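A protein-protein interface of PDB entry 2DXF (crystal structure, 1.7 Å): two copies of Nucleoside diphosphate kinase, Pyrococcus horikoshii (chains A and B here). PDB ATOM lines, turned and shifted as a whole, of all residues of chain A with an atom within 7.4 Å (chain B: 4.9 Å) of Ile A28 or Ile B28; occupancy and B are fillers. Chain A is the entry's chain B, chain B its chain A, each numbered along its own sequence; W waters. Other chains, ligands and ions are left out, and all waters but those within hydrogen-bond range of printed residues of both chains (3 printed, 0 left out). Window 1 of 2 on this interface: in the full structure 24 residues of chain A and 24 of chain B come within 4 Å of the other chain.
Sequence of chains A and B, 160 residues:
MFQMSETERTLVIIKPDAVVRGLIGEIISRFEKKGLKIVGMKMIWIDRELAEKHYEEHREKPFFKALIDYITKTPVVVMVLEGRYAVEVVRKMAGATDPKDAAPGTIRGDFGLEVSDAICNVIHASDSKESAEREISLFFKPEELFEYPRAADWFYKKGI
Among the printed residues, merely in contact across the chains: Ser A29 with Gly B25 (3.1 Å), Gly A25 with Ser B29 (3.1 Å), Gly A25 with Ile B28 (3.7 Å), Ile A28 with Gly B25 (3.7 Å), Ile A24 with Ile B38 (3.9 Å), Ile A38 with Ile B24 (3.9 Å), Ile A28 with Ile B28 (3.9 Å) and Val A77 with Met B41 (3.9 Å).
Ile A14 touches none of the printed residues of chain B. Of the printed residues of chain B, Gly A22 touches Glu B32. Ile A27 touches none of the printed residues of chain B. Of chain B, only Gly B25 (3.7 Å) and Ile B28 (3.9 Å) come within 4 Å of Ile A28. Of the printed residues of chain A, Ile B28 touches Gly A25 and Ile A28. The nearest residue of chain B that does not touch Ile A28 is Ile B24 (4.2 Å). The nearest residue of chain A that does not touch Ile B28 is Ile A24 (4.1 Å).
Gly A25 touches Ile B28, and with the chains exchanged Ile A28 touches Gly B25. Gly A25 touches Ser B29, and with the chains exchanged Ser A29 touches Gly B25. Gly A25 touches Glu B32, and with the chains exchanged Glu A32 touches Gly B25.
Water W2 lies within hydrogen-bond range of OE1 of Glu B32 (2.7 Å), OG of Ser B29 (2.8 Å), N of Glu A26 (3.0 Å), O of Gly A22 (3.0 Å) and N of Gly A25 (3.3 Å). Water W3 lies within hydrogen-bond range of OE1 of Glu A32, OG of Ser A29, N of Glu B26 and N of Gly B25.
The side-chain carboxylate of Glu A32 is in hydrogen-bond range of the backbone NH of Ile B24. N of Gly B25 lies within hydrogen-bond range of OE1 of Glu A32 (2.8 Å). OG of Ser A29 is in hydrogen-bond range of N of Glu B26, 3.0 Å away. OG of Ser B29 is in hydrogen-bond range of N of Glu A26, 3.0 Å away. The side-chain carboxylate (OE2) of Glu B32 is in hydrogen-bond range of the backbone NH (N) of Leu A23, at 3.4 Å. OE2 of Glu B32 sits at hydrogen-bond distance from N of Ile A24 (2.9 Å). OE1 of Glu B32 lies within hydrogen-bond range of N of Gly A25. The side-chain carboxylate (OE1) of Glu B32 sits close to the backbone carbonyl oxygen (O) of Gly A22, at 3.3 Å. O of Gly A25 lies close to O of Gly B25.
O of Gly B25 lies within hydrogen-bond range of OG of Ser B29 (3.2 Å). The backbone carbonyl oxygen of Val A77 lies within hydrogen-bond range of the backbone NH of Ile A14 (2.8 Å).
Printed residues of chain A that touch a printed residue of chain B: Gly A22, Leu A23, Ile A24, Gly A25, Glu A26, Ile A28, Ser A29, Glu A32, Ile A38 and Val A77. Hydrophobic or aromatic side chains of chain A within 4 Å of the printed part of chain B: Ile A24, Ile A28, Ile A38 and Val A77. Of the 13 printed residues of chain B, 8 touch a printed residue of chain A. Hydrophobic or aromatic side chains of chain B within 4 Å of the printed part of chain A: Ile B24, Ile B28, Ile B38 and Met B41. Along chain B the printed residues that touch a printed residue of chain A span positions 24 to 41. Among the printed residues, 17 pairs touch across the chains.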
ATOM      1  N   ILE A  14      18.404   0.458   3.545  1.00  0.00           N
ATOM      2  CA  ILE A  14      17.368   0.164   2.571  1.00  0.00           C
ATOM      3  C   ILE A  14      17.493  -1.353   2.457  1.00  0.00           C
ATOM      4  O   ILE A  14      18.415  -1.880   1.832  1.00  0.00           O
ATOM      5  CB  ILE A  14      17.638   0.865   1.225  1.00  0.00           C
ATOM      6  CG1 ILE A  14      17.573   2.380   1.437  1.00  0.00           C
ATOM      7  CG2 ILE A  14      16.604   0.426   0.187  1.00  0.00           C
ATOM      8  CD1 ILE A  14      17.839   3.213   0.193  1.00  0.00           C
ATOM      9  N   GLY A  22      13.157  -2.605  -6.483  1.00  0.00           N
ATOM     10  CA  GLY A  22      13.560  -1.415  -7.220  1.00  0.00           C
ATOM     11  C   GLY A  22      13.085  -0.107  -6.613  1.00  0.00           C
ATOM     12  O   GLY A  22      12.728   0.827  -7.338  1.00  0.00           O
ATOM     13  N   LEU A  23      13.111  -0.023  -5.288  1.00  0.00           N
ATOM     14  CA  LEU A  23      12.653   1.175  -4.589  1.00  0.00           C
ATOM     15  C   LEU A  23      13.749   2.047  -3.986  1.00  0.00           C
ATOM     16  O   LEU A  23      13.446   2.979  -3.237  1.00  0.00           O
ATOM     17  CB  LEU A  23      11.686   0.779  -3.472  1.00  0.00           C
ATOM     18  CG  LEU A  23      10.436   0.001  -3.878  1.00  0.00           C
ATOM     19  CD1 LEU A  23       9.669  -0.402  -2.626  1.00  0.00           C
ATOM     20  CD2 LEU A  23       9.572   0.851  -4.800  1.00  0.00           C
ATOM     21  N   ILE A  24      15.009   1.756  -4.294  1.00  0.00           N
ATOM     22  CA  ILE A  24      16.111   2.538  -3.732  1.00  0.00           C
ATOM     23  C   ILE A  24      15.971   4.032  -3.999  1.00  0.00           C
ATOM     24  O   ILE A  24      16.043   4.843  -3.078  1.00  0.00           O
ATOM     25  CB  ILE A  24      17.473   2.075  -4.296  1.00  0.00           C
ATOM     26  CG1 ILE A  24      17.769   0.646  -3.836  1.00  0.00           C
ATOM     27  CG2 ILE A  24      18.583   3.009  -3.827  1.00  0.00           C
ATOM     28  CD1 ILE A  24      19.022   0.056  -4.473  1.00  0.00           C
ATOM     29  N   GLY A  25      15.775   4.387  -5.264  1.00  0.00           N
ATOM     30  CA  GLY A  25      15.656   5.791  -5.623  1.00  0.00           C
ATOM     31  C   GLY A  25      14.515   6.542  -4.966  1.00  0.00           C
ATOM     32  O   GLY A  25      14.688   7.672  -4.505  1.00  0.00           O
ATOM     33  N   GLU A  26      13.339   5.925  -4.929  1.00  0.00           N
ATOM     34  CA  GLU A  26      12.174   6.563  -4.335  1.00  0.00           C
ATOM     35  C   GLU A  26      12.379   6.847  -2.856  1.00  0.00           C
ATOM     36  O   GLU A  26      11.953   7.890  -2.354  1.00  0.00           O
ATOM     37  CB  GLU A  26      10.940   5.688  -4.559  1.00  0.00           C
ATOM     38  CG  GLU A  26      10.581   5.565  -6.031  1.00  0.00           C
ATOM     39  CD  GLU A  26       9.596   4.450  -6.310  1.00  0.00           C
ATOM     40  OE1 GLU A  26       8.452   4.534  -5.829  1.00  0.00           O
ATOM     41  OE2 GLU A  26       9.974   3.486  -7.012  1.00  0.00           O
ATOM     42  N   ILE A  27      13.042   5.929  -2.162  1.00  0.00           N
ATOM     43  CA  ILE A  27      13.305   6.106  -0.740  1.00  0.00           C
ATOM     44  C   ILE A  27      14.297   7.243  -0.533  1.00  0.00           C
ATOM     45  O   ILE A  27      14.067   8.137   0.282  1.00  0.00           O
ATOM     46  CB  ILE A  27      13.848   4.800  -0.115  1.00  0.00           C
ATOM     47  CG1 ILE A  27      12.726   3.756  -0.085  1.00  0.00           C
ATOM     48  CG2 ILE A  27      14.377   5.066   1.293  1.00  0.00           C
ATOM     49  CD1 ILE A  27      13.205   2.326   0.121  1.00  0.00           C
ATOM     50  N   ILE A  28      15.391   7.224  -1.288  1.00  0.00           N
ATOM     51  CA  ILE A  28      16.392   8.272  -1.168  1.00  0.00           C
ATOM     52  C   ILE A  28      15.782   9.645  -1.462  1.00  0.00           C
ATOM     53  O   ILE A  28      16.046  10.604  -0.747  1.00  0.00           O
ATOM     54  CB  ILE A  28      17.595   8.012  -2.112  1.00  0.00           C
ATOM     55  CG1 ILE A  28      18.351   6.770  -1.633  1.00  0.00           C
ATOM     56  CG2 ILE A  28      18.513   9.236  -2.159  1.00  0.00           C
ATOM     57  CD1 ILE A  28      19.505   6.351  -2.525  1.00  0.00           C
ATOM     58  N   SER A  29      14.951   9.731  -2.496  1.00  0.00           N
ATOM     59  CA  SER A  29      14.325  11.006  -2.853  1.00  0.00           C
ATOM     60  C   SER A  29      13.495  11.596  -1.720  1.00  0.00           C
ATOM     61  O   SER A  29      13.410  12.815  -1.571  1.00  0.00           O
ATOM     62  CB  SER A  29      13.438  10.842  -4.088  1.00  0.00           C
ATOM     63  OG  SER A  29      14.215  10.638  -5.251  1.00  0.00           O
ATOM     64  N   ARG A  30      12.863  10.741  -0.924  1.00  0.00           N
ATOM     65  CA  ARG A  30      12.061  11.247   0.178  1.00  0.00           C
ATOM     66  C   ARG A  30      12.925  11.991   1.181  1.00  0.00           C
ATOM     67  O   ARG A  30      12.532  13.038   1.696  1.00  0.00           O
ATOM     68  CB  ARG A  30      11.323  10.105   0.864  1.00  0.00           C
ATOM     69  CG  ARG A  30      10.317   9.461  -0.056  1.00  0.00           C
ATOM     70  CD  ARG A  30       9.232   8.764   0.706  1.00  0.00           C
ATOM     71  NE  ARG A  30       8.195   8.291  -0.202  1.00  0.00           N
ATOM     72  CZ  ARG A  30       6.988   7.905   0.185  1.00  0.00           C
ATOM     73  NH1 ARG A  30       6.664   7.935   1.472  1.00  0.00           N
ATOM     74  NH2 ARG A  30       6.107   7.493  -0.719  1.00  0.00           N
ATOM     75  N   PHE A  31      14.108  11.449   1.452  1.00  0.00           N
ATOM     76  CA  PHE A  31      15.017  12.084   2.391  1.00  0.00           C
ATOM     77  C   PHE A  31      15.603  13.363   1.793  1.00  0.00           C
ATOM     78  O   PHE A  31      15.710  14.379   2.480  1.00  0.00           O
ATOM     79  CB  PHE A  31      16.133  11.112   2.783  1.00  0.00           C
ATOM     80  CG  PHE A  31      15.634   9.881   3.490  1.00  0.00           C
ATOM     81  CD1 PHE A  31      14.782   9.992   4.584  1.00  0.00           C
ATOM     82  CD2 PHE A  31      16.016   8.613   3.067  1.00  0.00           C
ATOM     83  CE1 PHE A  31      14.314   8.862   5.245  1.00  0.00           C
ATOM     84  CE2 PHE A  31      15.551   7.470   3.726  1.00  0.00           C
ATOM     85  CZ  PHE A  31      14.700   7.599   4.813  1.00  0.00           C
ATOM     86  N   GLU A  32      15.962  13.325   0.511  1.00  0.00           N
ATOM     87  CA  GLU A  32      16.515  14.511  -0.136  1.00  0.00           C
ATOM     88  C   GLU A  32      15.494  15.646  -0.173  1.00  0.00           C
ATOM     89  O   GLU A  32      15.829  16.793   0.098  1.00  0.00           O
ATOM     90  CB  GLU A  32      16.967  14.191  -1.562  1.00  0.00           C
ATOM     91  CG  GLU A  32      18.244  13.367  -1.646  1.00  0.00           C
ATOM     92  CD  GLU A  32      18.596  12.992  -3.073  1.00  0.00           C
ATOM     93  OE1 GLU A  32      17.786  12.283  -3.710  1.00  0.00           O
ATOM     94  OE2 GLU A  32      19.677  13.402  -3.558  1.00  0.00           O
ATOM     95  N   LYS A  33      14.249  15.313  -0.500  1.00  0.00           N
ATOM     96  CA  LYS A  33      13.179  16.305  -0.586  1.00  0.00           C
ATOM     97  C   LYS A  33      12.844  16.927   0.769  1.00  0.00           C
ATOM     98  O   LYS A  33      12.391  18.068   0.837  1.00  0.00           O
ATOM     99  CB  LYS A  33      11.930  15.663  -1.205  1.00  0.00           C
ATOM    100  CG  LYS A  33      10.762  16.617  -1.450  1.00  0.00           C
ATOM    101  CD  LYS A  33      11.152  17.812  -2.318  1.00  0.00           C
ATOM    102  CE  LYS A  33      11.683  17.389  -3.688  1.00  0.00           C
ATOM    103  NZ  LYS A  33      10.642  16.752  -4.537  1.00  0.00           N
ATOM    104  N   LYS A  34      13.077  16.177   1.843  1.00  0.00           N
ATOM    105  CA  LYS A  34      12.811  16.650   3.203  1.00  0.00           C
ATOM    106  C   LYS A  34      13.852  17.691   3.600  1.00  0.00           C
ATOM    107  O   LYS A  34      13.605  18.543   4.457  1.00  0.00           O
ATOM    108  CB  LYS A  34      12.864  15.462   4.176  1.00  0.00           C
ATOM    109  CG  LYS A  34      12.624  15.790   5.655  1.00  0.00           C
ATOM    110  CD  LYS A  34      11.206  16.278   5.922  1.00  0.00           C
ATOM    111  CE  LYS A  34      10.882  16.228   7.412  1.00  0.00           C
ATOM    112  NZ  LYS A  34       9.553  16.823   7.739  1.00  0.00           N
ATOM    113  N   LEU A  36      17.102  16.556   4.199  1.00  0.00           N
ATOM    114  CA  LEU A  36      18.149  15.775   4.853  1.00  0.00           C
ATOM    115  C   LEU A  36      19.321  15.605   3.894  1.00  0.00           C
ATOM    116  O   LEU A  36      19.134  15.507   2.685  1.00  0.00           O
ATOM    117  CB  LEU A  36      17.604  14.405   5.260  1.00  0.00           C
ATOM    118  CG  LEU A  36      16.612  14.413   6.426  1.00  0.00           C
ATOM    119  CD1 LEU A  36      15.821  13.117   6.428  1.00  0.00           C
ATOM    120  CD2 LEU A  36      17.365  14.605   7.746  1.00  0.00           C
ATOM    121  N   ILE A  38      22.694  13.461   2.609  1.00  0.00           N
ATOM    122  CA  ILE A  38      23.317  12.141   2.590  1.00  0.00           C
ATOM    123  C   ILE A  38      24.819  12.365   2.753  1.00  0.00           C
ATOM    124  O   ILE A  38      25.484  12.847   1.838  1.00  0.00           O
ATOM    125  CB  ILE A  38      23.070  11.415   1.255  1.00  0.00           C
ATOM    126  CG1 ILE A  38      21.567  11.254   1.023  1.00  0.00           C
ATOM    127  CG2 ILE A  38      23.772  10.053   1.265  1.00  0.00           C
ATOM    128  CD1 ILE A  38      21.210  10.878  -0.399  1.00  0.00           C
ATOM    129  N   MET A  41      27.065   6.736   1.992  1.00  0.00           N
ATOM    130  CA  MET A  41      26.194   5.745   1.369  1.00  0.00           C
ATOM    131  C   MET A  41      26.937   4.718   0.524  1.00  0.00           C
ATOM    132  O   MET A  41      27.914   5.032  -0.156  1.00  0.00           O
ATOM    133  CB  MET A  41      25.140   6.439   0.507  1.00  0.00           C
ATOM    134  CG  MET A  41      24.226   5.478  -0.222  1.00  0.00           C
ATOM    135  SD  MET A  41      22.857   6.325  -1.025  1.00  0.00           S
ATOM    136  CE  MET A  41      23.751   7.515  -2.012  1.00  0.00           C
ATOM    137  N   VAL A  77      21.373  -1.128   0.938  1.00  0.00           N
ATOM    138  CA  VAL A  77      22.015   0.165   0.775  1.00  0.00           C
ATOM    139  C   VAL A  77      22.020   0.806   2.149  1.00  0.00           C
ATOM    140  O   VAL A  77      20.963   1.077   2.718  1.00  0.00           O
ATOM    141  CB  VAL A  77      21.258   1.098  -0.203  1.00  0.00           C
ATOM    142  CG1 VAL A  77      21.899   2.480  -0.191  1.00  0.00           C
ATOM    143  CG2 VAL A  77      21.297   0.528  -1.602  1.00  0.00           C
ATOM    144  N   MET A  79      23.097   3.994   4.540  1.00  0.00           N
ATOM    145  CA  MET A  79      23.384   5.402   4.349  1.00  0.00           C
ATOM    146  C   MET A  79      23.223   6.190   5.629  1.00  0.00           C
ATOM    147  O   MET A  79      22.478   5.803   6.535  1.00  0.00           O
ATOM    148  CB  MET A  79      22.490   5.978   3.244  1.00  0.00           C
ATOM    149  CG  MET A  79      21.004   5.892   3.509  1.00  0.00           C
ATOM    150  SD  MET A  79      20.038   6.290   2.018  1.00  0.00           S
ATOM    151  CE  MET A  79      20.503   7.940   1.727  1.00  0.00           C
ATOM    152  N   LEU A  81      22.181   9.818   7.166  1.00  0.00           N
ATOM    153  CA  LEU A  81      21.456  11.049   6.875  1.00  0.00           C
ATOM    154  C   LEU A  81      21.758  12.076   7.948  1.00  0.00           C
ATOM    155  O   LEU A  81      21.724  11.771   9.138  1.00  0.00           O
ATOM    156  CB  LEU A  81      19.952  10.785   6.828  1.00  0.00           C
ATOM    157  CG  LEU A  81      19.525   9.815   5.724  1.00  0.00           C
ATOM    158  CD1 LEU A  81      18.046   9.502   5.861  1.00  0.00           C
ATOM    159  CD2 LEU A  81      19.825  10.427   4.358  1.00  0.00           C
ATOM    160  N   MET A  93       9.382   9.499   9.482  1.00  0.00           N
ATOM    161  CA  MET A  93       9.218   9.292   8.047  1.00  0.00           C
ATOM    162  C   MET A  93       9.060   7.809   7.721  1.00  0.00           C
ATOM    163  O   MET A  93       8.322   7.441   6.806  1.00  0.00           O
ATOM    164  CB  MET A  93      10.422   9.865   7.293  1.00  0.00           C
ATOM    165  CG  MET A  93      10.518  11.379   7.348  1.00  0.00           C
ATOM    166  SD  MET A  93      11.959  11.994   6.451  1.00  0.00           S
ATOM    167  CE  MET A  93      11.507  11.559   4.750  1.00  0.00           C
ATOM    168  N   ILE A 107       7.147   5.967   4.652  1.00  0.00           N
ATOM    169  CA  ILE A 107       7.794   5.023   3.750  1.00  0.00           C
ATOM    170  C   ILE A 107       7.195   3.622   3.879  1.00  0.00           C
ATOM    171  O   ILE A 107       6.841   2.995   2.885  1.00  0.00           O
ATOM    172  CB  ILE A 107       9.312   4.974   4.020  1.00  0.00           C
ATOM    173  CG1 ILE A 107       9.934   6.318   3.625  1.00  0.00           C
ATOM    174  CG2 ILE A 107       9.959   3.841   3.233  1.00  0.00           C
ATOM    175  CD1 ILE A 107      11.359   6.494   4.099  1.00  0.00           C
ATOM    176  N   PHE A 111       4.937   1.862   0.947  1.00  0.00           N
ATOM    177  CA  PHE A 111       5.618   0.764   0.259  1.00  0.00           C
ATOM    178  C   PHE A 111       5.585  -0.627   0.876  1.00  0.00           C
ATOM    179  O   PHE A 111       5.844  -1.609   0.174  1.00  0.00           O
ATOM    180  CB  PHE A 111       7.097   1.126   0.053  1.00  0.00           C
ATOM    181  CG  PHE A 111       7.326   2.442  -0.641  1.00  0.00           C
ATOM    182  CD1 PHE A 111       8.484   3.168  -0.388  1.00  0.00           C
ATOM    183  CD2 PHE A 111       6.411   2.946  -1.559  1.00  0.00           C
ATOM    184  CE1 PHE A 111       8.732   4.379  -1.038  1.00  0.00           C
ATOM    185  CE2 PHE A 111       6.651   4.157  -2.214  1.00  0.00           C
ATOM    186  CZ  PHE A 111       7.813   4.870  -1.952  1.00  0.00           C
ATOM    187  N   ARG A 150      24.867  21.336   0.615  1.00  0.00           N
ATOM    188  CA  ARG A 150      23.763  20.983  -0.262  1.00  0.00           C
ATOM    189  C   ARG A 150      23.347  22.350  -0.797  1.00  0.00           C
ATOM    190  O   ARG A 150      23.680  23.376  -0.203  1.00  0.00           O
ATOM    191  CB  ARG A 150      22.632  20.305   0.512  1.00  0.00           C
ATOM    192  CG  ARG A 150      22.708  18.776   0.459  1.00  0.00           C
ATOM    193  CD  ARG A 150      22.137  18.245  -0.853  1.00  0.00           C
ATOM    194  NE  ARG A 150      20.694  18.459  -0.896  1.00  0.00           N
ATOM    195  CZ  ARG A 150      19.806  17.658  -0.316  1.00  0.00           C
ATOM    196  NH1 ARG A 150      20.212  16.576   0.339  1.00  0.00           N
ATOM    197  NH2 ARG A 150      18.516  17.960  -0.351  1.00  0.00           N
ATOM    198  N   ILE B  14      26.982  10.044 -10.482  1.00  0.00           N
ATOM    199  CA  ILE B  14      26.007  11.094 -10.232  1.00  0.00           C
ATOM    200  C   ILE B  14      26.910  12.241  -9.786  1.00  0.00           C
ATOM    201  O   ILE B  14      27.457  12.235  -8.685  1.00  0.00           O
ATOM    202  CB  ILE B  14      25.006  10.682  -9.135  1.00  0.00           C
ATOM    203  CG1 ILE B  14      24.185   9.488  -9.640  1.00  0.00           C
ATOM    204  CG2 ILE B  14      24.093  11.855  -8.790  1.00  0.00           C
ATOM    205  CD1 ILE B  14      23.173   8.932  -8.636  1.00  0.00           C
ATOM    206  N   ILE B  24      19.825  12.651  -6.378  1.00  0.00           N
ATOM    207  CA  ILE B  24      20.341  11.283  -6.387  1.00  0.00           C
ATOM    208  C   ILE B  24      19.231  10.251  -6.540  1.00  0.00           C
ATOM    209  O   ILE B  24      19.294   9.373  -7.404  1.00  0.00           O
ATOM    210  CB  ILE B  24      21.128  10.974  -5.092  1.00  0.00           C
ATOM    211  CG1 ILE B  24      22.342  11.903  -4.992  1.00  0.00           C
ATOM    212  CG2 ILE B  24      21.580   9.506  -5.088  1.00  0.00           C
ATOM    213  CD1 ILE B  24      23.131  11.761  -3.696  1.00  0.00           C
ATOM    214  N   GLY B  25      18.211  10.370  -5.696  1.00  0.00           N
ATOM    215  CA  GLY B  25      17.108   9.428  -5.734  1.00  0.00           C
ATOM    216  C   GLY B  25      16.368   9.381  -7.059  1.00  0.00           C
ATOM    217  O   GLY B  25      16.086   8.302  -7.582  1.00  0.00           O
ATOM    218  N   GLU B  26      16.053  10.552  -7.604  1.00  0.00           N
ATOM    219  CA  GLU B  26      15.331  10.627  -8.872  1.00  0.00           C
ATOM    220  C   GLU B  26      16.112   9.979 -10.013  1.00  0.00           C
ATOM    221  O   GLU B  26      15.536   9.300 -10.865  1.00  0.00           O
ATOM    222  CB  GLU B  26      15.012  12.089  -9.200  1.00  0.00           C
ATOM    223  CG  GLU B  26      14.029  12.719  -8.221  1.00  0.00           C
ATOM    224  CD  GLU B  26      13.889  14.221  -8.398  1.00  0.00           C
ATOM    225  OE1 GLU B  26      13.450  14.655  -9.480  1.00  0.00           O
ATOM    226  OE2 GLU B  26      14.222  14.965  -7.449  1.00  0.00           O
ATOM    227  N   ILE B  27      17.426  10.174 -10.021  1.00  0.00           N
ATOM    228  CA  ILE B  27      18.262   9.589 -11.059  1.00  0.00           C
ATOM    229  C   ILE B  27      18.278   8.067 -10.911  1.00  0.00           C
ATOM    230  O   ILE B  27      18.046   7.340 -11.876  1.00  0.00           O
ATOM    231  CB  ILE B  27      19.700  10.160 -10.982  1.00  0.00           C
ATOM    232  CG1 ILE B  27      19.660  11.655 -11.302  1.00  0.00           C
ATOM    233  CG2 ILE B  27      20.622   9.430 -11.959  1.00  0.00           C
ATOM    234  CD1 ILE B  27      20.975  12.384 -11.059  1.00  0.00           C
ATOM    235  N   ILE B  28      18.515   7.585  -9.696  1.00  0.00           N
ATOM    236  CA  ILE B  28      18.546   6.143  -9.467  1.00  0.00           C
ATOM    237  C   ILE B  28      17.215   5.500  -9.865  1.00  0.00           C
ATOM    238  O   ILE B  28      17.193   4.452 -10.511  1.00  0.00           O
ATOM    239  CB  ILE B  28      18.861   5.820  -7.985  1.00  0.00           C
ATOM    240  CG1 ILE B  28      20.325   6.162  -7.696  1.00  0.00           C
ATOM    241  CG2 ILE B  28      18.573   4.349  -7.684  1.00  0.00           C
ATOM    242  CD1 ILE B  28      20.718   6.040  -6.244  1.00  0.00           C
ATOM    243  N   SER B  29      16.109   6.140  -9.503  1.00  0.00           N
ATOM    244  CA  SER B  29      14.789   5.605  -9.830  1.00  0.00           C
ATOM    245  C   SER B  29      14.580   5.386 -11.322  1.00  0.00           C
ATOM    246  O   SER B  29      13.930   4.427 -11.726  1.00  0.00           O
ATOM    247  CB  SER B  29      13.694   6.530  -9.298  1.00  0.00           C
ATOM    248  OG  SER B  29      13.575   6.396  -7.898  1.00  0.00           O
ATOM    249  N   ARG B  30      15.123   6.274 -12.148  1.00  0.00           N
ATOM    250  CA  ARG B  30      14.962   6.112 -13.584  1.00  0.00           C
ATOM    251  C   ARG B  30      15.605   4.812 -14.051  1.00  0.00           C
ATOM    252  O   ARG B  30      15.074   4.127 -14.922  1.00  0.00           O
ATOM    253  CB  ARG B  30      15.566   7.303 -14.324  1.00  0.00           C
ATOM    254  CG  ARG B  30      14.845   8.589 -14.001  1.00  0.00           C
ATOM    255  CD  ARG B  30      15.002   9.610 -15.090  1.00  0.00           C
ATOM    256  NE  ARG B  30      14.204  10.796 -14.805  1.00  0.00           N
ATOM    257  CZ  ARG B  30      13.930  11.741 -15.696  1.00  0.00           C
ATOM    258  NH1 ARG B  30      14.391  11.635 -16.935  1.00  0.00           N
ATOM    259  NH2 ARG B  30      13.200  12.790 -15.343  1.00  0.00           N
ATOM    260  N   PHE B  31      16.742   4.468 -13.460  1.00  0.00           N
ATOM    261  CA  PHE B  31      17.431   3.240 -13.826  1.00  0.00           C
ATOM    262  C   PHE B  31      16.670   2.020 -13.313  1.00  0.00           C
ATOM    263  O   PHE B  31      16.480   1.045 -14.040  1.00  0.00           O
ATOM    264  CB  PHE B  31      18.864   3.265 -13.287  1.00  0.00           C
ATOM    265  CG  PHE B  31      19.702   4.371 -13.869  1.00  0.00           C
ATOM    266  CD1 PHE B  31      19.729   4.583 -15.248  1.00  0.00           C
ATOM    267  CD2 PHE B  31      20.452   5.209 -13.047  1.00  0.00           C
ATOM    268  CE1 PHE B  31      20.489   5.611 -15.799  1.00  0.00           C
ATOM    269  CE2 PHE B  31      21.218   6.244 -13.595  1.00  0.00           C
ATOM    270  CZ  PHE B  31      21.233   6.442 -14.969  1.00  0.00           C
ATOM    271  N   GLU B  32      16.211   2.075 -12.067  1.00  0.00           N
ATOM    272  CA  GLU B  32      15.457   0.959 -11.510  1.00  0.00           C
ATOM    273  C   GLU B  32      14.164   0.712 -12.290  1.00  0.00           C
ATOM    274  O   GLU B  32      13.814  -0.434 -12.572  1.00  0.00           O
ATOM    275  CB  GLU B  32      15.119   1.224 -10.041  1.00  0.00           C
ATOM    276  CG  GLU B  32      16.310   1.152  -9.098  1.00  0.00           C
ATOM    277  CD  GLU B  32      15.934   1.526  -7.673  1.00  0.00           C
ATOM    278  OE1 GLU B  32      15.512   2.680  -7.455  1.00  0.00           O
ATOM    279  OE2 GLU B  32      16.059   0.668  -6.776  1.00  0.00           O
ATOM    280  N   ILE B  38      21.243  -2.384 -10.010  1.00  0.00           N
ATOM    281  CA  ILE B  38      22.383  -1.719  -9.382  1.00  0.00           C
ATOM    282  C   ILE B  38      23.208  -2.827  -8.738  1.00  0.00           C
ATOM    283  O   ILE B  38      22.783  -3.427  -7.753  1.00  0.00           O
ATOM    284  CB  ILE B  38      21.933  -0.730  -8.287  1.00  0.00           C
ATOM    285  CG1 ILE B  38      21.076   0.372  -8.910  1.00  0.00           C
ATOM    286  CG2 ILE B  38      23.153  -0.131  -7.583  1.00  0.00           C
ATOM    287  CD1 ILE B  38      20.394   1.260  -7.890  1.00  0.00           C
ATOM    288  N   MET B  41      27.490   0.381  -5.750  1.00  0.00           N
ATOM    289  CA  MET B  41      27.211   1.794  -5.512  1.00  0.00           C
ATOM    290  C   MET B  41      27.815   2.342  -4.231  1.00  0.00           C
ATOM    291  O   MET B  41      27.820   1.681  -3.195  1.00  0.00           O
ATOM    292  CB  MET B  41      25.698   2.038  -5.492  1.00  0.00           C
ATOM    293  CG  MET B  41      25.317   3.486  -5.238  1.00  0.00           C
ATOM    294  SD  MET B  41      23.573   3.802  -5.575  1.00  0.00           S
ATOM    295  CE  MET B  41      22.827   3.146  -4.096  1.00  0.00           C
ATOM    296  N   MET B  79      28.188   4.325  -9.378  1.00  0.00           N
ATOM    297  CA  MET B  79      27.389   3.116  -9.335  1.00  0.00           C
ATOM    298  C   MET B  79      27.531   2.326 -10.617  1.00  0.00           C
ATOM    299  O   MET B  79      27.788   2.883 -11.686  1.00  0.00           O
ATOM    300  CB  MET B  79      25.919   3.468  -9.080  1.00  0.00           C
ATOM    301  CG  MET B  79      25.257   4.264 -10.183  1.00  0.00           C
ATOM    302  SD  MET B  79      23.638   4.903  -9.669  1.00  0.00           S
ATOM    303  CE  MET B  79      22.728   3.448  -9.446  1.00  0.00           C
HETATM  304  O   HOH W   1      12.823   8.934  -7.013  1.00  0.00           O
HETATM  305  O   HOH W   2      13.070   3.811  -7.061  1.00  0.00           O
HETATM  306  O   HOH W   3      15.918  12.821  -5.706  1.00  0.00           O
